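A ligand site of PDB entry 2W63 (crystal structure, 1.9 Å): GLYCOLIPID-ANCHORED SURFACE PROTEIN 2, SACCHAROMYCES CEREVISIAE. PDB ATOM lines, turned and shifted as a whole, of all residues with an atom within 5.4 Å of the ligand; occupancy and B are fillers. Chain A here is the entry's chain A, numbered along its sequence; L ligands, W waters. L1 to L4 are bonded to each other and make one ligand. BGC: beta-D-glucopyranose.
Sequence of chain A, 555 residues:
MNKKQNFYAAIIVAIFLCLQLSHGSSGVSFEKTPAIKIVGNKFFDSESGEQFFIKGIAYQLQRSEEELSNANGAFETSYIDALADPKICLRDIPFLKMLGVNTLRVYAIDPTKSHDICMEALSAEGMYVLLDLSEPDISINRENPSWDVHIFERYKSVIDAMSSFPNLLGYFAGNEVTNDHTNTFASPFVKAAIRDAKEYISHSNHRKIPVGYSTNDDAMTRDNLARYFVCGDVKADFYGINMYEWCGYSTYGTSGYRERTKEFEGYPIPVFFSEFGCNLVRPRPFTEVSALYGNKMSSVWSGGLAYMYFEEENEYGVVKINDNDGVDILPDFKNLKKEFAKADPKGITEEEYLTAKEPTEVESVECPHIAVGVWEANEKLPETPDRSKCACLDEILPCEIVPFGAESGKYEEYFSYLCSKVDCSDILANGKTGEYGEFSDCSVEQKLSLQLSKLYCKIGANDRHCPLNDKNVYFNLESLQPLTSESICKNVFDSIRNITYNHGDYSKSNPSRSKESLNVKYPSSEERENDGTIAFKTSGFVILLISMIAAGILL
OG of Ser 139 lies within hydrogen-bond range of O4 of BGC L2, at 2.9 Å.
NE2 of Gln 62 sits at hydrogen-bond distance from O6 of BGC L1, at 2.6 Å.
The backbone NH (N) of Arg 142 sits at hydrogen-bond distance from an oxygen (O4) of BGC L3, 3.1 Å away.
The side-chain amide nitrogen (ND2) of Asn 141 lies within hydrogen-bond range of an oxygen (O3) of BGC L4 (3.4 Å).
O4 of BGC L2 sits at hydrogen-bond distance from OG of Ser 134 (2.7 Å).
The backbone carbonyl oxygen (O) of Ser 134 sits at hydrogen-bond distance from an oxygen (O6) of BGC L2, 3.2 Å away.
The side-chain hydroxyl (OH) of Tyr 307 is in hydrogen-bond range of an oxygen (O5) of BGC L1 (3.0 Å).
The side-chain amide nitrogen (ND2) of Asn 175 sits at hydrogen-bond distance from an oxygen (O2) of BGC L1 (3.2 Å).
The guanidinium group (NH1) of Arg 142 is in hydrogen-bond range of an oxygen (O6) of BGC L4 (2.9 Å).
O6 of BGC L2 sits at hydrogen-bond distance from O of Tyr 107 (2.5 Å).
O of Pro 136 lies within hydrogen-bond range of O2 of BGC L3 (3.0 Å).
The backbone carbonyl oxygen (O) of Ile 140 is in hydrogen-bond range of an oxygen (O6) of BGC L3 (2.7 Å).
OE2 of Glu 275 is in hydrogen-bond range of OH of Tyr 107 (2.7 Å).
NE2 of Gln 62 sits at hydrogen-bond distance from OE1 of Glu 312 (3.1 Å).
The side-chain hydroxyl of Ser 139 sits at hydrogen-bond distance from the backbone carbonyl oxygen of Glu 135 (2.5 Å).
The backbone NH of Tyr 107 is in hydrogen-bond range of the side-chain amide oxygen of Gln 60 (2.8 Å).
N of Glu 143 is in hydrogen-bond range of OD1 of Asn 141.
The guanidinium group (NH2) of Arg 142 is in hydrogen-bond range of the backbone carbonyl oxygen (O) of Glu 176, 2.8 Å away.
N of Asp 137 lies within hydrogen-bond range of OE1 of Glu 135 (2.9 Å).
O of Val 177 is in hydrogen-bond range of NE of Arg 142 (2.8 Å).
CB of Asp 132 touches C6 of BGC L2, at 3.7 Å.
CA of Glu 135 touches O6 of BGC L2, 3.5 Å away.
CG of Glu 143 touches C6 of BGC L4, at 3.7 Å.
CG2 of Val 177 touches O6 of BGC L3, 3.5 Å away.
Glu 275 touches the ligand.
Water W10 lies within hydrogen-bond range of O6 of BGC L4 and OE2 of Glu 143.
Water W1 lies within hydrogen-bond range of OE1 of Glu 275 and O1 of BGC L1.
Water W4 lies within hydrogen-bond range of an oxygen (O6) of BGC L3 and the backbone NH (N) of Asn 175.
Water W11 lies within hydrogen-bond range of the side-chain carboxylate (OE2) of Glu 275 (2.5 Å), an oxygen (O1) of BGC L1 (3.0 Å) and the side-chain amide nitrogen (ND2) of Asn 175 (3.3 Å).
Water W5 bridges O of Pro 136 (2.7 Å) and O2 of BGC L4 (3.2 Å).
Water W2 lies within hydrogen-bond range of the side-chain amide nitrogen (ND2) of Asn 141 and an oxygen (O3) of BGC L4.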
ATOM      1  N   GLN A  60      16.522  26.716  10.149  1.00  0.00           N
ATOM      2  CA  GLN A  60      17.144  25.429  10.429  1.00  0.00           C
ATOM      3  C   GLN A  60      16.368  24.322   9.755  1.00  0.00           C
ATOM      4  O   GLN A  60      15.156  24.128   9.997  1.00  0.00           O
ATOM      5  CB  GLN A  60      17.232  25.156  11.953  1.00  0.00           C
ATOM      6  CG  GLN A  60      18.058  23.906  12.308  1.00  0.00           C
ATOM      7  CD  GLN A  60      19.547  24.178  12.287  1.00  0.00           C
ATOM      8  OE1 GLN A  60      19.979  25.252  12.691  1.00  0.00           O
ATOM      9  NE2 GLN A  60      20.327  23.236  11.774  1.00  0.00           N
ATOM     10  N   GLN A  62      15.843  20.272   8.841  1.00  0.00           N
ATOM     11  CA  GLN A  62      15.760  19.102   9.710  1.00  0.00           C
ATOM     12  C   GLN A  62      15.557  17.838   8.885  1.00  0.00           C
ATOM     13  O   GLN A  62      16.528  17.267   8.373  1.00  0.00           O
ATOM     14  CB  GLN A  62      14.585  19.262  10.689  1.00  0.00           C
ATOM     15  CG  GLN A  62      14.995  19.476  12.138  1.00  0.00           C
ATOM     16  CD  GLN A  62      15.235  20.928  12.572  1.00  0.00           C
ATOM     17  OE1 GLN A  62      16.010  21.161  13.526  1.00  0.00           O
ATOM     18  NE2 GLN A  62      14.563  21.896  11.919  1.00  0.00           N
ATOM     19  N   TYR A 107      20.251  26.738  15.031  1.00  0.00           N
ATOM     20  CA  TYR A 107      20.324  25.881  16.213  1.00  0.00           C
ATOM     21  C   TYR A 107      21.503  24.917  16.165  1.00  0.00           C
ATOM     22  O   TYR A 107      21.900  24.362  17.199  1.00  0.00           O
ATOM     23  CB  TYR A 107      19.035  25.072  16.362  1.00  0.00           C
ATOM     24  CG  TYR A 107      17.796  25.895  16.607  1.00  0.00           C
ATOM     25  CD1 TYR A 107      17.111  26.490  15.526  1.00  0.00           C
ATOM     26  CD2 TYR A 107      17.298  26.064  17.896  1.00  0.00           C
ATOM     27  CE1 TYR A 107      15.952  27.225  15.733  1.00  0.00           C
ATOM     28  CE2 TYR A 107      16.130  26.803  18.132  1.00  0.00           C
ATOM     29  CZ  TYR A 107      15.468  27.408  17.035  1.00  0.00           C
ATOM     30  OH  TYR A 107      14.302  28.151  17.229  1.00  0.00           O
ATOM     31  N   ALA A 108      22.034  24.677  14.981  1.00  0.00           N
ATOM     32  CA  ALA A 108      23.135  23.721  14.843  1.00  0.00           C
ATOM     33  C   ALA A 108      23.993  24.036  13.630  1.00  0.00           C
ATOM     34  O   ALA A 108      23.467  24.144  12.509  1.00  0.00           O
ATOM     35  CB  ALA A 108      22.608  22.283  14.735  1.00  0.00           C
ATOM     36  N   ASP A 132      23.039  28.667  18.554  1.00  0.00           N
ATOM     37  CA  ASP A 132      23.265  27.711  19.640  1.00  0.00           C
ATOM     38  C   ASP A 132      24.633  27.030  19.549  1.00  0.00           C
ATOM     39  O   ASP A 132      25.116  26.725  18.451  1.00  0.00           O
ATOM     40  CB  ASP A 132      22.162  26.649  19.710  1.00  0.00           C
ATOM     41  CG  ASP A 132      20.802  27.276  19.905  1.00  0.00           C
ATOM     42  OD1 ASP A 132      20.315  27.904  18.950  1.00  0.00           O
ATOM     43  OD2 ASP A 132      20.202  27.158  21.001  1.00  0.00           O
ATOM     44  N   SER A 134      25.256  24.132  21.211  1.00  0.00           N
ATOM     45  CA  SER A 134      24.997  22.697  21.298  1.00  0.00           C
ATOM     46  C   SER A 134      24.435  22.148  19.974  1.00  0.00           C
ATOM     47  O   SER A 134      24.198  22.896  19.004  1.00  0.00           O
ATOM     48  CB  SER A 134      24.030  22.403  22.472  1.00  0.00           C
ATOM     49  OG  SER A 134      22.777  23.079  22.304  1.00  0.00           O
ATOM     50  N   GLU A 135      24.267  20.837  19.940  1.00  0.00           N
ATOM     51  CA  GLU A 135      23.560  20.186  18.865  1.00  0.00           C
ATOM     52  C   GLU A 135      22.822  18.990  19.497  1.00  0.00           C
ATOM     53  O   GLU A 135      23.127  18.635  20.647  1.00  0.00           O
ATOM     54  CB  GLU A 135      24.518  19.810  17.712  1.00  0.00           C
ATOM     55  CG  GLU A 135      25.705  18.921  18.072  1.00  0.00           C
ATOM     56  CD  GLU A 135      25.556  17.480  17.645  1.00  0.00           C
ATOM     57  OE1 GLU A 135      24.410  16.977  17.478  1.00  0.00           O
ATOM     58  OE2 GLU A 135      26.599  16.811  17.497  1.00  0.00           O
ATOM     59  N   PRO A 136      21.802  18.420  18.797  1.00  0.00           N
ATOM     60  CA  PRO A 136      20.909  17.469  19.487  1.00  0.00           C
ATOM     61  C   PRO A 136      21.621  16.286  20.167  1.00  0.00           C
ATOM     62  O   PRO A 136      21.148  15.819  21.218  1.00  0.00           O
ATOM     63  CB  PRO A 136      20.015  16.959  18.355  1.00  0.00           C
ATOM     64  CG  PRO A 136      19.985  18.067  17.371  1.00  0.00           C
ATOM     65  CD  PRO A 136      21.380  18.662  17.408  1.00  0.00           C
ATOM     66  N   ASP A 137      22.718  15.818  19.569  1.00  0.00           N
ATOM     67  CA  ASP A 137      23.476  14.676  20.079  1.00  0.00           C
ATOM     68  C   ASP A 137      24.530  15.095  21.094  1.00  0.00           C
ATOM     69  O   ASP A 137      25.100  14.241  21.775  1.00  0.00           O
ATOM     70  CB  ASP A 137      24.133  13.923  18.910  1.00  0.00           C
ATOM     71  CG  ASP A 137      23.115  13.182  18.029  1.00  0.00           C
ATOM     72  OD1 ASP A 137      21.952  13.030  18.431  1.00  0.00           O
ATOM     73  OD2 ASP A 137      23.510  12.732  16.918  1.00  0.00           O
ATOM     74  N   SER A 139      24.449  17.971  23.932  1.00  0.00           N
ATOM     75  CA  SER A 139      23.712  19.013  24.660  1.00  0.00           C
ATOM     76  C   SER A 139      23.675  18.602  26.115  1.00  0.00           C
ATOM     77  O   SER A 139      23.817  17.417  26.446  1.00  0.00           O
ATOM     78  CB  SER A 139      22.260  19.065  24.179  1.00  0.00           C
ATOM     79  OG  SER A 139      22.161  19.456  22.829  1.00  0.00           O
ATOM     80  N   ILE A 140      23.432  19.556  27.007  1.00  0.00           N
ATOM     81  CA  ILE A 140      23.262  19.212  28.411  1.00  0.00           C
ATOM     82  C   ILE A 140      21.943  18.460  28.554  1.00  0.00           C
ATOM     83  O   ILE A 140      20.905  18.947  28.109  1.00  0.00           O
ATOM     84  CB  ILE A 140      23.288  20.469  29.327  1.00  0.00           C
ATOM     85  CG1 ILE A 140      24.678  21.136  29.238  1.00  0.00           C
ATOM     86  CG2 ILE A 140      22.920  20.087  30.774  1.00  0.00           C
ATOM     87  CD1 ILE A 140      24.708  22.573  29.742  1.00  0.00           C
ATOM     88  N   ASN A 141      22.000  17.248  29.103  1.00  0.00           N
ATOM     89  CA  ASN A 141      20.835  16.351  29.176  1.00  0.00           C
ATOM     90  C   ASN A 141      19.978  16.835  30.351  1.00  0.00           C
ATOM     91  O   ASN A 141      20.386  16.738  31.506  1.00  0.00           O
ATOM     92  CB  ASN A 141      21.320  14.892  29.377  1.00  0.00           C
ATOM     93  CG  ASN A 141      20.178  13.889  29.470  1.00  0.00           C
ATOM     94  OD1 ASN A 141      19.122  14.187  29.995  1.00  0.00           O
ATOM     95  ND2 ASN A 141      20.422  12.663  28.991  1.00  0.00           N
ATOM     96  N   ARG A 142      18.780  17.356  30.061  1.00  0.00           N
ATOM     97  CA  ARG A 142      17.986  17.965  31.137  1.00  0.00           C
ATOM     98  C   ARG A 142      17.571  16.962  32.226  1.00  0.00           C
ATOM     99  O   ARG A 142      17.352  17.358  33.380  1.00  0.00           O
ATOM    100  CB  ARG A 142      16.779  18.733  30.603  1.00  0.00           C
ATOM    101  CG  ARG A 142      15.763  17.883  29.873  1.00  0.00           C
ATOM    102  CD  ARG A 142      14.518  18.669  29.484  1.00  0.00           C
ATOM    103  NE  ARG A 142      14.736  19.615  28.378  1.00  0.00           N
ATOM    104  CZ  ARG A 142      14.722  19.299  27.073  1.00  0.00           C
ATOM    105  NH1 ARG A 142      14.573  18.024  26.659  1.00  0.00           N
ATOM    106  NH2 ARG A 142      14.862  20.257  26.173  1.00  0.00           N
ATOM    107  N   GLU A 143      17.465  15.682  31.880  1.00  0.00           N
ATOM    108  CA  GLU A 143      17.033  14.703  32.875  1.00  0.00           C
ATOM    109  C   GLU A 143      18.176  14.103  33.687  1.00  0.00           C
ATOM    110  O   GLU A 143      17.982  13.719  34.853  1.00  0.00           O
ATOM    111  CB  GLU A 143      16.133  13.622  32.273  1.00  0.00           C
ATOM    112  CG  GLU A 143      14.778  14.132  31.709  1.00  0.00           C
ATOM    113  CD  GLU A 143      13.903  14.909  32.749  1.00  0.00           C
ATOM    114  OE1 GLU A 143      13.873  14.532  33.960  1.00  0.00           O
ATOM    115  OE2 GLU A 143      13.218  15.882  32.336  1.00  0.00           O
ATOM    116  N   ASN A 175      19.315  25.818  25.428  1.00  0.00           N
ATOM    117  CA  ASN A 175      17.972  26.108  24.946  1.00  0.00           C
ATOM    118  C   ASN A 175      16.977  25.209  25.659  1.00  0.00           C
ATOM    119  O   ASN A 175      16.986  23.995  25.450  1.00  0.00           O
ATOM    120  CB  ASN A 175      17.895  25.845  23.444  1.00  0.00           C
ATOM    121  CG  ASN A 175      16.490  26.108  22.902  1.00  0.00           C
ATOM    122  OD1 ASN A 175      15.913  27.156  23.152  1.00  0.00           O
ATOM    123  ND2 ASN A 175      15.928  25.142  22.177  1.00  0.00           N
ATOM    124  N   GLU A 176      16.114  25.803  26.491  1.00  0.00           N
ATOM    125  CA  GLU A 176      15.029  25.075  27.197  1.00  0.00           C
ATOM    126  C   GLU A 176      15.558  23.792  27.838  1.00  0.00           C
ATOM    127  O   GLU A 176      15.029  22.699  27.584  1.00  0.00           O
ATOM    128  CB  GLU A 176      13.876  24.721  26.226  1.00  0.00           C
ATOM    129  CG  GLU A 176      13.406  25.852  25.347  1.00  0.00           C
ATOM    130  CD  GLU A 176      12.102  25.503  24.653  1.00  0.00           C
ATOM    131  OE1 GLU A 176      11.822  24.281  24.487  1.00  0.00           O
ATOM    132  OE2 GLU A 176      11.354  26.445  24.286  1.00  0.00           O
ATOM    133  N   VAL A 177      16.615  23.913  28.634  1.00  0.00           N
ATOM    134  CA  VAL A 177      17.202  22.751  29.291  1.00  0.00           C
ATOM    135  C   VAL A 177      16.274  22.369  30.456  1.00  0.00           C
ATOM    136  O   VAL A 177      15.498  21.447  30.322  1.00  0.00           O
ATOM    137  CB  VAL A 177      18.679  23.006  29.692  1.00  0.00           C
ATOM    138  CG1 VAL A 177      19.300  21.772  30.316  1.00  0.00           C
ATOM    139  CG2 VAL A 177      19.503  23.492  28.428  1.00  0.00           C
ATOM    140  N   GLU A 275      11.852  32.881  20.167  1.00  0.00           N
ATOM    141  CA  GLU A 275      10.865  32.346  19.209  1.00  0.00           C
ATOM    142  C   GLU A 275       9.554  33.080  19.461  1.00  0.00           C
ATOM    143  O   GLU A 275       9.252  33.424  20.604  1.00  0.00           O
ATOM    144  CB  GLU A 275      10.622  30.817  19.397  1.00  0.00           C
ATOM    145  CG  GLU A 275      11.781  29.906  18.913  1.00  0.00           C
ATOM    146  CD  GLU A 275      11.722  28.458  19.418  1.00  0.00           C
ATOM    147  OE1 GLU A 275      10.606  27.993  19.808  1.00  0.00           O
ATOM    148  OE2 GLU A 275      12.804  27.805  19.409  1.00  0.00           O
ATOM    149  N   TYR A 307       9.226  31.890  14.471  1.00  0.00           N
ATOM    150  CA  TYR A 307       9.533  30.474  14.236  1.00  0.00           C
ATOM    151  C   TYR A 307       8.558  29.906  13.190  1.00  0.00           C
ATOM    152  O   TYR A 307       7.368  29.805  13.482  1.00  0.00           O
ATOM    153  CB  TYR A 307       9.416  29.674  15.550  1.00  0.00           C
ATOM    154  CG  TYR A 307       9.878  28.250  15.400  1.00  0.00           C
ATOM    155  CD1 TYR A 307       8.992  27.265  14.940  1.00  0.00           C
ATOM    156  CD2 TYR A 307      11.221  27.903  15.644  1.00  0.00           C
ATOM    157  CE1 TYR A 307       9.415  25.952  14.753  1.00  0.00           C
ATOM    158  CE2 TYR A 307      11.651  26.584  15.471  1.00  0.00           C
ATOM    159  CZ  TYR A 307      10.733  25.627  15.029  1.00  0.00           C
ATOM    160  OH  TYR A 307      11.144  24.328  14.869  1.00  0.00           O
ATOM    161  N   MET A 308       9.023  29.523  11.989  1.00  0.00           N
ATOM    162  CA  MET A 308      10.404  29.645  11.482  1.00  0.00           C
ATOM    163  C   MET A 308      10.355  29.726   9.940  1.00  0.00           C
ATOM    164  O   MET A 308       9.270  29.733   9.333  1.00  0.00           O
ATOM    165  CB  MET A 308      11.262  28.432  11.918  1.00  0.00           C
ATOM    166  CG  MET A 308      10.916  27.079  11.224  1.00  0.00           C
ATOM    167  SD  MET A 308      12.438  26.086  10.913  1.00  0.00           S
ATOM    168  CE  MET A 308      13.377  27.054   9.833  1.00  0.00           C
ATOM    169  N   GLU A 312       8.080  22.233   7.996  1.00  0.00           N
ATOM    170  CA  GLU A 312       8.422  20.832   8.216  1.00  0.00           C
ATOM    171  C   GLU A 312       7.273  19.964   8.726  1.00  0.00           C
ATOM    172  O   GLU A 312       7.441  19.215   9.684  1.00  0.00           O
ATOM    173  CB  GLU A 312       9.617  20.747   9.156  1.00  0.00           C
ATOM    174  CG  GLU A 312      10.864  20.414   8.380  1.00  0.00           C
ATOM    175  CD  GLU A 312      12.055  21.172   8.841  1.00  0.00           C
ATOM    176  OE1 GLU A 312      12.089  21.612  10.011  1.00  0.00           O
ATOM    177  OE2 GLU A 312      12.963  21.317   8.004  1.00  0.00           O
HETATM  178  C2  BGC L   1      14.090  22.836  18.951  1.00  0.00           C
HETATM  179  C3  BGC L   1      15.487  22.679  18.343  1.00  0.00           C
HETATM  180  C4  BGC L   1      15.411  22.586  16.812  1.00  0.00           C
HETATM  181  C5  BGC L   1      14.649  23.814  16.269  1.00  0.00           C
HETATM  182  C6  BGC L   1      14.551  23.902  14.742  1.00  0.00           C
HETATM  183  C1  BGC L   1      13.305  23.958  18.264  1.00  0.00           C
HETATM  184  O1  BGC L   1      11.960  23.984  18.776  1.00  0.00           O
HETATM  185  O2  BGC L   1      14.220  23.090  20.355  1.00  0.00           O
HETATM  186  O3  BGC L   1      16.039  21.444  18.817  1.00  0.00           O
HETATM  187  O4  BGC L   1      16.727  22.423  16.231  1.00  0.00           O
HETATM  188  O5  BGC L   1      13.303  23.742  16.803  1.00  0.00           O
HETATM  189  O6  BGC L   1      13.792  22.808  14.273  1.00  0.00           O
HETATM  190  C2  BGC L   2      17.384  20.268  20.418  1.00  0.00           C
HETATM  191  C3  BGC L   2      18.438  20.457  21.523  1.00  0.00           C
HETATM  192  C4  BGC L   2      19.650  21.298  21.059  1.00  0.00           C
HETATM  193  C5  BGC L   2      19.176  22.596  20.339  1.00  0.00           C
HETATM  194  C6  BGC L   2      20.339  23.430  19.731  1.00  0.00           C
HETATM  195  C1  BGC L   2      17.030  21.639  19.815  1.00  0.00           C
HETATM  196  O2  BGC L   2      16.212  19.596  20.962  1.00  0.00           O
HETATM  197  O3  BGC L   2      18.893  19.159  21.866  1.00  0.00           O
HETATM  198  O4  BGC L   2      20.442  21.654  22.195  1.00  0.00           O
HETATM  199  O5  BGC L   2      18.249  22.224  19.266  1.00  0.00           O
HETATM  200  O6  BGC L   2      21.034  22.623  18.773  1.00  0.00           O
HETATM  201  C2  BGC L   3      18.855  17.312  23.399  1.00  0.00           C
HETATM  202  C3  BGC L   3      18.356  16.841  24.771  1.00  0.00           C
HETATM  203  C4  BGC L   3      18.601  17.848  25.873  1.00  0.00           C
HETATM  204  C5  BGC L   3      18.092  19.228  25.450  1.00  0.00           C
HETATM  205  C6  BGC L   3      18.439  20.281  26.507  1.00  0.00           C
HETATM  206  C1  BGC L   3      18.310  18.696  23.092  1.00  0.00           C
HETATM  207  O2  BGC L   3      18.458  16.394  22.395  1.00  0.00           O
HETATM  208  O3  BGC L   3      19.084  15.684  25.146  1.00  0.00           O
HETATM  209  O4  BGC L   3      17.941  17.415  27.091  1.00  0.00           O
HETATM  210  O5  BGC L   3      18.731  19.541  24.197  1.00  0.00           O
HETATM  211  O6  BGC L   3      19.800  20.651  26.369  1.00  0.00           O
HETATM  212  C2  BGC L   4      18.991  13.330  25.616  1.00  0.00           C
HETATM  213  C3  BGC L   4      18.074  12.164  25.993  1.00  0.00           C
HETATM  214  C4  BGC L   4      17.150  12.538  27.169  1.00  0.00           C
HETATM  215  C5  BGC L   4      16.421  13.875  26.900  1.00  0.00           C
HETATM  216  C6  BGC L   4      15.670  14.315  28.169  1.00  0.00           C
HETATM  217  C1  BGC L   4      18.174  14.606  25.420  1.00  0.00           C
HETATM  218  O2  BGC L   4      19.652  13.009  24.399  1.00  0.00           O
HETATM  219  O3  BGC L   4      18.893  11.048  26.362  1.00  0.00           O
HETATM  220  O4  BGC L   4      16.184  11.492  27.368  1.00  0.00           O
HETATM  221  O5  BGC L   4      17.371  14.912  26.591  1.00  0.00           O
HETATM  222  O6  BGC L   4      14.760  15.362  27.820  1.00  0.00           O
HETATM  223  O   HOH W   1      10.187  25.651  20.157  1.00  0.00           O
HETATM  224  O   HOH W   2      18.628  10.662  29.743  1.00  0.00           O
HETATM  225  O   HOH W   3      19.108  21.319  16.559  1.00  0.00           O
HETATM  226  O   HOH W   4      20.517  23.047  25.010  1.00  0.00           O
HETATM  227  O   HOH W   5      22.063  14.871  23.519  1.00  0.00           O
HETATM  228  O   HOH W   6      14.395  10.827  25.350  1.00  0.00           O
HETATM  229  O   HOH W   7      12.093  21.165  15.610  1.00  0.00           O
HETATM  230  O   HOH W   8      16.448  16.992  20.150  1.00  0.00           O
HETATM  231  O   HOH W   9      16.445  22.499  23.329  1.00  0.00           O
HETATM  232  O   HOH W  10      12.789  15.326  29.615  1.00  0.00           O
HETATM  233  O   HOH W  11      12.985  25.815  20.968  1.00  0.00           O
